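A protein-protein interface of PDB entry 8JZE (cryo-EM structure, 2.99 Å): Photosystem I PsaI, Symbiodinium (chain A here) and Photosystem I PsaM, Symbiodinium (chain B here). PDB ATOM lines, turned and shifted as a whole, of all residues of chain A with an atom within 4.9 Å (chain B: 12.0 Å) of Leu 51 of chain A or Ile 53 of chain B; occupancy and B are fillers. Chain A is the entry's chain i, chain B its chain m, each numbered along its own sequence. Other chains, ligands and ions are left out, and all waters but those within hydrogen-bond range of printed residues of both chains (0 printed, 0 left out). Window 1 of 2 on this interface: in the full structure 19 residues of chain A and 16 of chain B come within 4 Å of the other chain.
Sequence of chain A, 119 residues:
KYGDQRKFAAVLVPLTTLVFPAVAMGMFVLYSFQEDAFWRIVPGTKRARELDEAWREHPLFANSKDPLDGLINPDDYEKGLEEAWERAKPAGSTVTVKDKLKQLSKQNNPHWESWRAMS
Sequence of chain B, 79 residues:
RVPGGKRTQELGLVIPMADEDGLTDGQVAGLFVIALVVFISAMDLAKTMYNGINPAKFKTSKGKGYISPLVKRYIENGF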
ATOM      1  N   TRP A  39       7.308 -17.615   0.888  1.00  0.00           N
ATOM      2  CA  TRP A  39       8.378 -16.870   0.237  1.00  0.00           C
ATOM      3  C   TRP A  39       9.447 -17.763  -0.377  1.00  0.00           C
ATOM      4  O   TRP A  39      10.257 -17.267  -1.167  1.00  0.00           O
ATOM      5  CB  TRP A  39       9.029 -15.911   1.234  1.00  0.00           C
ATOM      6  CG  TRP A  39       9.824 -16.592   2.299  1.00  0.00           C
ATOM      7  CD1 TRP A  39       9.356 -17.103   3.473  1.00  0.00           C
ATOM      8  CD2 TRP A  39      11.236 -16.826   2.293  1.00  0.00           C
ATOM      9  NE1 TRP A  39      10.390 -17.647   4.197  1.00  0.00           N
ATOM     10  CE2 TRP A  39      11.555 -17.489   3.493  1.00  0.00           C
ATOM     11  CE3 TRP A  39      12.261 -16.542   1.387  1.00  0.00           C
ATOM     12  CZ2 TRP A  39      12.855 -17.872   3.810  1.00  0.00           C
ATOM     13  CZ3 TRP A  39      13.550 -16.923   1.703  1.00  0.00           C
ATOM     14  CH2 TRP A  39      13.836 -17.579   2.904  1.00  0.00           C
ATOM     15  N   ARG A  47      11.238 -11.163   1.025  1.00  0.00           N
ATOM     16  CA  ARG A  47      12.240 -11.899   1.786  1.00  0.00           C
ATOM     17  C   ARG A  47      13.179 -12.674   0.874  1.00  0.00           C
ATOM     18  O   ARG A  47      14.357 -12.843   1.202  1.00  0.00           O
ATOM     19  CB  ARG A  47      11.555 -12.839   2.778  1.00  0.00           C
ATOM     20  CG  ARG A  47      12.497 -13.476   3.785  1.00  0.00           C
ATOM     21  CD  ARG A  47      11.735 -14.279   4.829  1.00  0.00           C
ATOM     22  NE  ARG A  47      10.746 -13.470   5.530  1.00  0.00           N
ATOM     23  CZ  ARG A  47      10.990 -12.758   6.622  1.00  0.00           C
ATOM     24  NH1 ARG A  47      12.193 -12.725   7.171  1.00  0.00           N
ATOM     25  NH2 ARG A  47      10.002 -12.062   7.176  1.00  0.00           N
ATOM     26  N   ALA A  48      12.684 -13.150  -0.271  1.00  0.00           N
ATOM     27  CA  ALA A  48      13.559 -13.830  -1.221  1.00  0.00           C
ATOM     28  C   ALA A  48      14.635 -12.888  -1.745  1.00  0.00           C
ATOM     29  O   ALA A  48      15.811 -13.265  -1.838  1.00  0.00           O
ATOM     30  CB  ALA A  48      12.737 -14.406  -2.374  1.00  0.00           C
ATOM     31  N   ARG A  49      14.251 -11.657  -2.089  1.00  0.00           N
ATOM     32  CA  ARG A  49      15.228 -10.670  -2.533  1.00  0.00           C
ATOM     33  C   ARG A  49      16.244 -10.380  -1.442  1.00  0.00           C
ATOM     34  O   ARG A  49      17.453 -10.310  -1.703  1.00  0.00           O
ATOM     35  CB  ARG A  49      14.530  -9.375  -2.940  1.00  0.00           C
ATOM     36  CG  ARG A  49      13.589  -9.478  -4.110  1.00  0.00           C
ATOM     37  CD  ARG A  49      13.133  -8.085  -4.485  1.00  0.00           C
ATOM     38  NE  ARG A  49      12.125  -8.087  -5.534  1.00  0.00           N
ATOM     39  CZ  ARG A  49      11.613  -6.991  -6.074  1.00  0.00           C
ATOM     40  NH1 ARG A  49      12.003  -5.785  -5.695  1.00  0.00           N
ATOM     41  NH2 ARG A  49      10.684  -7.108  -7.014  1.00  0.00           N
ATOM     42  N   GLU A  50      15.768 -10.187  -0.210  1.00  0.00           N
ATOM     43  CA  GLU A  50      16.694  -9.878   0.875  1.00  0.00           C
ATOM     44  C   GLU A  50      17.660 -11.028   1.118  1.00  0.00           C
ATOM     45  O   GLU A  50      18.850 -10.804   1.360  1.00  0.00           O
ATOM     46  CB  GLU A  50      15.933  -9.532   2.153  1.00  0.00           C
ATOM     47  CG  GLU A  50      15.776  -8.039   2.379  1.00  0.00           C
ATOM     48  CD  GLU A  50      14.644  -7.447   1.572  1.00  0.00           C
ATOM     49  OE1 GLU A  50      13.516  -7.961   1.688  1.00  0.00           O
ATOM     50  OE2 GLU A  50      14.880  -6.476   0.822  1.00  0.00           O
ATOM     51  N   LEU A  51      17.171 -12.267   1.049  1.00  0.00           N
ATOM     52  CA  LEU A  51      18.041 -13.421   1.249  1.00  0.00           C
ATOM     53  C   LEU A  51      19.074 -13.542   0.137  1.00  0.00           C
ATOM     54  O   LEU A  51      20.248 -13.834   0.401  1.00  0.00           O
ATOM     55  CB  LEU A  51      17.203 -14.695   1.348  1.00  0.00           C
ATOM     56  CG  LEU A  51      16.947 -15.215   2.763  1.00  0.00           C
ATOM     57  CD1 LEU A  51      18.241 -15.724   3.378  1.00  0.00           C
ATOM     58  CD2 LEU A  51      16.322 -14.136   3.639  1.00  0.00           C
ATOM     59  N   ASP A  52      18.660 -13.327  -1.115  1.00  0.00           N
ATOM     60  CA  ASP A  52      19.615 -13.390  -2.217  1.00  0.00           C
ATOM     61  C   ASP A  52      20.688 -12.317  -2.075  1.00  0.00           C
ATOM     62  O   ASP A  52      21.880 -12.589  -2.268  1.00  0.00           O
ATOM     63  CB  ASP A  52      18.891 -13.254  -3.556  1.00  0.00           C
ATOM     64  CG  ASP A  52      18.021 -14.454  -3.875  1.00  0.00           C
ATOM     65  OD1 ASP A  52      17.807 -15.293  -2.974  1.00  0.00           O
ATOM     66  OD2 ASP A  52      17.556 -14.562  -5.029  1.00  0.00           O
ATOM     67  N   GLU A  53      20.287 -11.094  -1.720  1.00  0.00           N
ATOM     68  CA  GLU A  53      21.269 -10.029  -1.547  1.00  0.00           C
ATOM     69  C   GLU A  53      22.183 -10.304  -0.359  1.00  0.00           C
ATOM     70  O   GLU A  53      23.381 -10.003  -0.409  1.00  0.00           O
ATOM     71  CB  GLU A  53      20.562  -8.681  -1.397  1.00  0.00           C
ATOM     72  CG  GLU A  53      19.882  -8.209  -2.674  1.00  0.00           C
ATOM     73  CD  GLU A  53      19.082  -6.935  -2.483  1.00  0.00           C
ATOM     74  OE1 GLU A  53      18.946  -6.480  -1.328  1.00  0.00           O
ATOM     75  OE2 GLU A  53      18.586  -6.390  -3.492  1.00  0.00           O
ATOM     76  N   ALA A  54      21.639 -10.881   0.717  1.00  0.00           N
ATOM     77  CA  ALA A  54      22.467 -11.244   1.862  1.00  0.00           C
ATOM     78  C   ALA A  54      23.504 -12.289   1.478  1.00  0.00           C
ATOM     79  O   ALA A  54      24.656 -12.221   1.920  1.00  0.00           O
ATOM     80  CB  ALA A  54      21.590 -11.753   3.005  1.00  0.00           C
ATOM     81  N   TRP A  55      23.109 -13.272   0.667  1.00  0.00           N
ATOM     82  CA  TRP A  55      24.083 -14.233   0.161  1.00  0.00           C
ATOM     83  C   TRP A  55      25.142 -13.546  -0.690  1.00  0.00           C
ATOM     84  O   TRP A  55      26.333 -13.856  -0.583  1.00  0.00           O
ATOM     85  CB  TRP A  55      23.384 -15.333  -0.639  1.00  0.00           C
ATOM     86  CG  TRP A  55      22.912 -16.473   0.202  1.00  0.00           C
ATOM     87  CD1 TRP A  55      21.623 -16.881   0.386  1.00  0.00           C
ATOM     88  CD2 TRP A  55      23.727 -17.354   0.980  1.00  0.00           C
ATOM     89  NE1 TRP A  55      21.587 -17.964   1.229  1.00  0.00           N
ATOM     90  CE2 TRP A  55      22.867 -18.273   1.609  1.00  0.00           C
ATOM     91  CE3 TRP A  55      25.102 -17.452   1.210  1.00  0.00           C
ATOM     92  CZ2 TRP A  55      23.337 -19.276   2.451  1.00  0.00           C
ATOM     93  CZ3 TRP A  55      25.565 -18.449   2.045  1.00  0.00           C
ATOM     94  CH2 TRP A  55      24.686 -19.349   2.654  1.00  0.00           C
ATOM     95  N   ASP B  44      10.544 -23.754  17.930  1.00  0.00           N
ATOM     96  CA  ASP B  44      11.756 -22.985  17.658  1.00  0.00           C
ATOM     97  C   ASP B  44      12.492 -23.525  16.434  1.00  0.00           C
ATOM     98  O   ASP B  44      12.955 -22.753  15.582  1.00  0.00           O
ATOM     99  CB  ASP B  44      12.666 -23.003  18.886  1.00  0.00           C
ATOM    100  CG  ASP B  44      13.923 -22.174  18.700  1.00  0.00           C
ATOM    101  OD1 ASP B  44      13.941 -21.291  17.816  1.00  0.00           O
ATOM    102  OD2 ASP B  44      14.896 -22.410  19.443  1.00  0.00           O
ATOM    103  N   LEU B  45      12.609 -24.851  16.333  1.00  0.00           N
ATOM    104  CA  LEU B  45      13.286 -25.453  15.190  1.00  0.00           C
ATOM    105  C   LEU B  45      12.541 -25.164  13.894  1.00  0.00           C
ATOM    106  O   LEU B  45      13.161 -24.930  12.851  1.00  0.00           O
ATOM    107  CB  LEU B  45      13.428 -26.960  15.395  1.00  0.00           C
ATOM    108  CG  LEU B  45      14.251 -27.654  14.313  1.00  0.00           C
ATOM    109  CD1 LEU B  45      15.665 -27.121  14.358  1.00  0.00           C
ATOM    110  CD2 LEU B  45      14.231 -29.162  14.477  1.00  0.00           C
ATOM    111  N   ALA B  46      11.208 -25.199  13.937  1.00  0.00           N
ATOM    112  CA  ALA B  46      10.419 -24.874  12.757  1.00  0.00           C
ATOM    113  C   ALA B  46      10.648 -23.433  12.330  1.00  0.00           C
ATOM    114  O   ALA B  46      10.771 -23.145  11.135  1.00  0.00           O
ATOM    115  CB  ALA B  46       8.936 -25.130  13.026  1.00  0.00           C
ATOM    116  N   LYS B  47      10.716 -22.512  13.297  1.00  0.00           N
ATOM    117  CA  LYS B  47      11.026 -21.124  12.965  1.00  0.00           C
ATOM    118  C   LYS B  47      12.389 -21.014  12.292  1.00  0.00           C
ATOM    119  O   LYS B  47      12.540 -20.336  11.266  1.00  0.00           O
ATOM    120  CB  LYS B  47      10.985 -20.255  14.223  1.00  0.00           C
ATOM    121  CG  LYS B  47       9.596 -19.951  14.755  1.00  0.00           C
ATOM    122  CD  LYS B  47       9.658 -18.865  15.820  1.00  0.00           C
ATOM    123  CE  LYS B  47       8.275 -18.510  16.342  1.00  0.00           C
ATOM    124  NZ  LYS B  47       7.619 -19.672  16.999  1.00  0.00           N
ATOM    125  N   THR B  48      13.397 -21.683  12.858  1.00  0.00           N
ATOM    126  CA  THR B  48      14.749 -21.579  12.313  1.00  0.00           C
ATOM    127  C   THR B  48      14.828 -22.166  10.908  1.00  0.00           C
ATOM    128  O   THR B  48      15.492 -21.603  10.030  1.00  0.00           O
ATOM    129  CB  THR B  48      15.749 -22.270  13.236  1.00  0.00           C
ATOM    130  OG1 THR B  48      15.550 -21.817  14.581  1.00  0.00           O
ATOM    131  CG2 THR B  48      17.166 -21.938  12.811  1.00  0.00           C
ATOM    132  N   MET B  49      14.160 -23.298  10.677  1.00  0.00           N
ATOM    133  CA  MET B  49      14.150 -23.894   9.345  1.00  0.00           C
ATOM    134  C   MET B  49      13.391 -23.023   8.352  1.00  0.00           C
ATOM    135  O   MET B  49      13.783 -22.920   7.184  1.00  0.00           O
ATOM    136  CB  MET B  49      13.545 -25.296   9.395  1.00  0.00           C
ATOM    137  CG  MET B  49      14.561 -26.418   9.356  1.00  0.00           C
ATOM    138  SD  MET B  49      13.790 -28.042   9.452  1.00  0.00           S
ATOM    139  CE  MET B  49      12.751 -27.834  10.895  1.00  0.00           C
ATOM    140  N   TYR B  50      12.294 -22.402   8.791  1.00  0.00           N
ATOM    141  CA  TYR B  50      11.530 -21.529   7.907  1.00  0.00           C
ATOM    142  C   TYR B  50      12.359 -20.328   7.477  1.00  0.00           C
ATOM    143  O   TYR B  50      12.395 -19.973   6.294  1.00  0.00           O
ATOM    144  CB  TYR B  50      10.248 -21.079   8.603  1.00  0.00           C
ATOM    145  CG  TYR B  50       9.402 -20.115   7.804  1.00  0.00           C
ATOM    146  CD1 TYR B  50       8.562 -20.572   6.797  1.00  0.00           C
ATOM    147  CD2 TYR B  50       9.430 -18.751   8.066  1.00  0.00           C
ATOM    148  CE1 TYR B  50       7.782 -19.698   6.069  1.00  0.00           C
ATOM    149  CE2 TYR B  50       8.654 -17.870   7.341  1.00  0.00           C
ATOM    150  CZ  TYR B  50       7.832 -18.349   6.344  1.00  0.00           C
ATOM    151  OH  TYR B  50       7.055 -17.476   5.620  1.00  0.00           O
ATOM    152  N   ASN B  51      13.040 -19.687   8.430  1.00  0.00           N
ATOM    153  CA  ASN B  51      13.832 -18.512   8.085  1.00  0.00           C
ATOM    154  C   ASN B  51      15.144 -18.876   7.403  1.00  0.00           C
ATOM    155  O   ASN B  51      15.648 -18.095   6.590  1.00  0.00           O
ATOM    156  CB  ASN B  51      14.098 -17.669   9.332  1.00  0.00           C
ATOM    157  CG  ASN B  51      12.838 -17.030   9.879  1.00  0.00           C
ATOM    158  OD1 ASN B  51      12.278 -16.118   9.273  1.00  0.00           O
ATOM    159  ND2 ASN B  51      12.388 -17.504  11.034  1.00  0.00           N
ATOM    160  N   GLY B  52      15.712 -20.037   7.713  1.00  0.00           N
ATOM    161  CA  GLY B  52      16.937 -20.460   7.070  1.00  0.00           C
ATOM    162  C   GLY B  52      18.161 -19.739   7.606  1.00  0.00           C
ATOM    163  O   GLY B  52      18.106 -18.956   8.559  1.00  0.00           O
ATOM    164  N   ILE B  53      19.295 -20.014   6.958  1.00  0.00           N
ATOM    165  CA  ILE B  53      20.561 -19.428   7.379  1.00  0.00           C
ATOM    166  C   ILE B  53      20.591 -17.950   7.016  1.00  0.00           C
ATOM    167  O   ILE B  53      20.092 -17.537   5.961  1.00  0.00           O
ATOM    168  CB  ILE B  53      21.743 -20.170   6.734  1.00  0.00           C
ATOM    169  CG1 ILE B  53      21.458 -21.668   6.648  1.00  0.00           C
ATOM    170  CG2 ILE B  53      23.019 -19.924   7.525  1.00  0.00           C
ATOM    171  CD1 ILE B  53      22.462 -22.418   5.807  1.00  0.00           C
ATOM    172  N   ASN B  54      21.185 -17.145   7.892  1.00  0.00           N
ATOM    173  CA  ASN B  54      21.392 -15.728   7.620  1.00  0.00           C
ATOM    174  C   ASN B  54      22.872 -15.484   7.370  1.00  0.00           C
ATOM    175  O   ASN B  54      23.665 -15.492   8.325  1.00  0.00           O
ATOM    176  CB  ASN B  54      20.895 -14.870   8.784  1.00  0.00           C
ATOM    177  CG  ASN B  54      19.425 -15.085   9.081  1.00  0.00           C
ATOM    178  OD1 ASN B  54      18.560 -14.404   8.529  1.00  0.00           O
ATOM    179  ND2 ASN B  54      19.133 -16.037   9.960  1.00  0.00           N
ATOM    180  N   PRO B  55      23.295 -15.274   6.126  1.00  0.00           N
ATOM    181  CA  PRO B  55      24.728 -15.103   5.848  1.00  0.00           C
ATOM    182  C   PRO B  55      25.247 -13.742   6.276  1.00  0.00           C
ATOM    183  O   PRO B  55      26.434 -13.591   6.581  1.00  0.00           O
ATOM    184  CB  PRO B  55      24.816 -15.275   4.325  1.00  0.00           C
ATOM    185  CG  PRO B  55      23.483 -15.817   3.902  1.00  0.00           C
ATOM    186  CD  PRO B  55      22.499 -15.317   4.893  1.00  0.00           C
ATOM    187  N   ALA B  56      24.366 -12.746   6.299  1.00  0.00           N
ATOM    188  CA  ALA B  56      24.737 -11.376   6.622  1.00  0.00           C
ATOM    189  C   ALA B  56      24.948 -11.151   8.115  1.00  0.00           C
ATOM    190  O   ALA B  56      25.038  -9.996   8.544  1.00  0.00           O
ATOM    191  CB  ALA B  56      23.674 -10.406   6.097  1.00  0.00           C
ATOM    192  N   LYS B  57      25.027 -12.220   8.910  1.00  0.00           N
ATOM    193  CA  LYS B  57      25.224 -12.065  10.347  1.00  0.00           C
ATOM    194  C   LYS B  57      26.599 -11.497  10.672  1.00  0.00           C
ATOM    195  O   LYS B  57      26.763 -10.830  11.700  1.00  0.00           O
ATOM    196  CB  LYS B  57      25.024 -13.405  11.053  1.00  0.00           C
ATOM    197  CG  LYS B  57      23.585 -13.892  11.054  1.00  0.00           C
ATOM    198  CD  LYS B  57      22.709 -13.033  11.950  1.00  0.00           C
ATOM    199  CE  LYS B  57      23.062 -13.235  13.413  1.00  0.00           C
ATOM    200  NZ  LYS B  57      22.933 -14.664  13.812  1.00  0.00           N
ATOM    201  N   PHE B  58      27.592 -11.737   9.814  1.00  0.00           N
ATOM    202  CA  PHE B  58      28.940 -11.253  10.082  1.00  0.00           C
ATOM    203  C   PHE B  58      29.034  -9.734  10.072  1.00  0.00           C
ATOM    204  O   PHE B  58      30.028  -9.189  10.564  1.00  0.00           O
ATOM    205  CB  PHE B  58      29.927 -11.845   9.070  1.00  0.00           C
ATOM    206  CG  PHE B  58      29.863 -11.218   7.706  1.00  0.00           C
ATOM    207  CD1 PHE B  58      28.923 -11.635   6.779  1.00  0.00           C
ATOM    208  CD2 PHE B  58      30.762 -10.226   7.342  1.00  0.00           C
ATOM    209  CE1 PHE B  58      28.869 -11.065   5.522  1.00  0.00           C
ATOM    210  CE2 PHE B  58      30.712  -9.652   6.087  1.00  0.00           C
ATOM    211  CZ  PHE B  58      29.765 -10.073   5.176  1.00  0.00           C
ATOM    212  N   LYS B  59      28.034  -9.041   9.527  1.00  0.00           N
ATOM    213  CA  LYS B  59      28.037  -7.584   9.547  1.00  0.00           C
ATOM    214  C   LYS B  59      27.504  -7.023  10.859  1.00  0.00           C
ATOM    215  O   LYS B  59      27.894  -5.920  11.256  1.00  0.00           O
ATOM    216  CB  LYS B  59      27.213  -7.036   8.379  1.00  0.00           C
ATOM    217  CG  LYS B  59      27.858  -7.205   7.012  1.00  0.00           C
ATOM    218  CD  LYS B  59      27.118  -6.392   5.958  1.00  0.00           C
ATOM    219  CE  LYS B  59      27.908  -6.303   4.660  1.00  0.00           C
ATOM    220  NZ  LYS B  59      28.055  -7.627   3.998  1.00  0.00           N
ATOM    221  N   THR B  60      26.626  -7.753  11.542  1.00  0.00           N
ATOM    222  CA  THR B  60      25.972  -7.252  12.747  1.00  0.00           C
ATOM    223  C   THR B  60      26.247  -8.087  13.987  1.00  0.00           C
ATOM    224  O   THR B  60      26.459  -7.522  15.063  1.00  0.00           O
ATOM    225  CB  THR B  60      24.453  -7.165  12.531  1.00  0.00           C
ATOM    226  OG1 THR B  60      23.924  -8.474  12.293  1.00  0.00           O
ATOM    227  CG2 THR B  60      24.131  -6.268  11.345  1.00  0.00           C
ATOM    228  N   SER B  61      26.244  -9.412  13.872  1.00  0.00           N
ATOM    229  CA  SER B  61      26.421 -10.266  15.040  1.00  0.00           C
ATOM    230  C   SER B  61      27.819 -10.102  15.627  1.00  0.00           C
ATOM    231  O   SER B  61      28.788  -9.820  14.918  1.00  0.00           O
ATOM    232  CB  SER B  61      26.179 -11.731  14.673  1.00  0.00           C
ATOM    233  OG  SER B  61      26.345 -12.574  15.799  1.00  0.00           O
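Of the printed residues of chain B, Arg 47 of chain A touches Asn 51. No residue of chain B comes within 4 Å of Ala 48 of chain A. No residue of chain B comes within 4 Å of Glu 50 of chain A. Leu 51 of chain A touches one residue of chain B. Asp 52 of chain A touches none of the printed residues of chain B. Glu 53 of chain A touches none of the printed residues of chain B. Of the printed residues of chain B, Ala 54 of chain A touches Pro 55 (3.9 Å) and Ala 56 (3.96 Å). Of chain B, only Pro 55 (3.3 Å) comes within 4 Å of Trp 55 of chain A. Of the printed residues of chain A, Pro 55 of chain B touches Ala 54 and Trp 55. The nearest residue of chain A that does not touch Ile 53 of chain B is Trp 55 of chain A (4.7 Å).
Printed residues of chain B that touch a printed residue of chain A: Tyr 50, Asn 51, Ile 53, Pro 55 and Ala 56. Hydrophobic or aromatic side chains of chain B within 4 Å of the printed part of chain A: Tyr 50, Pro 55 and Ala 56. Of the 10 printed residues of chain A, 5 touch a printed residue of chain B. Printed residues of chain A that touch a printed residue of chain B: Trp 39, Arg 47, Leu 51, Ala 54 and Trp 55. Among the printed residues, 7 pairs touch across the chains.
ND2 of Asn 51 of chain B is in hydrogen-bond range of O of Lys 47 of chain B, at 2.8 Å.
CD1 of Trp 39 of chain A touches OH of Tyr 50 of chain B (3.2 Å). Trp 39 of chain A touches Asn 51 of chain B. Arg 47 of chain A touches Asn 51 of chain B. Ile 53 of chain B touches Leu 51 of chain A. Ala 54 of chain A touches Pro 55 of chain B (O to CB, 3.9 Å). Ala 56 of chain B touches Ala 54 of chain A. Pro 55 of chain B touches Trp 55 of chain A.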
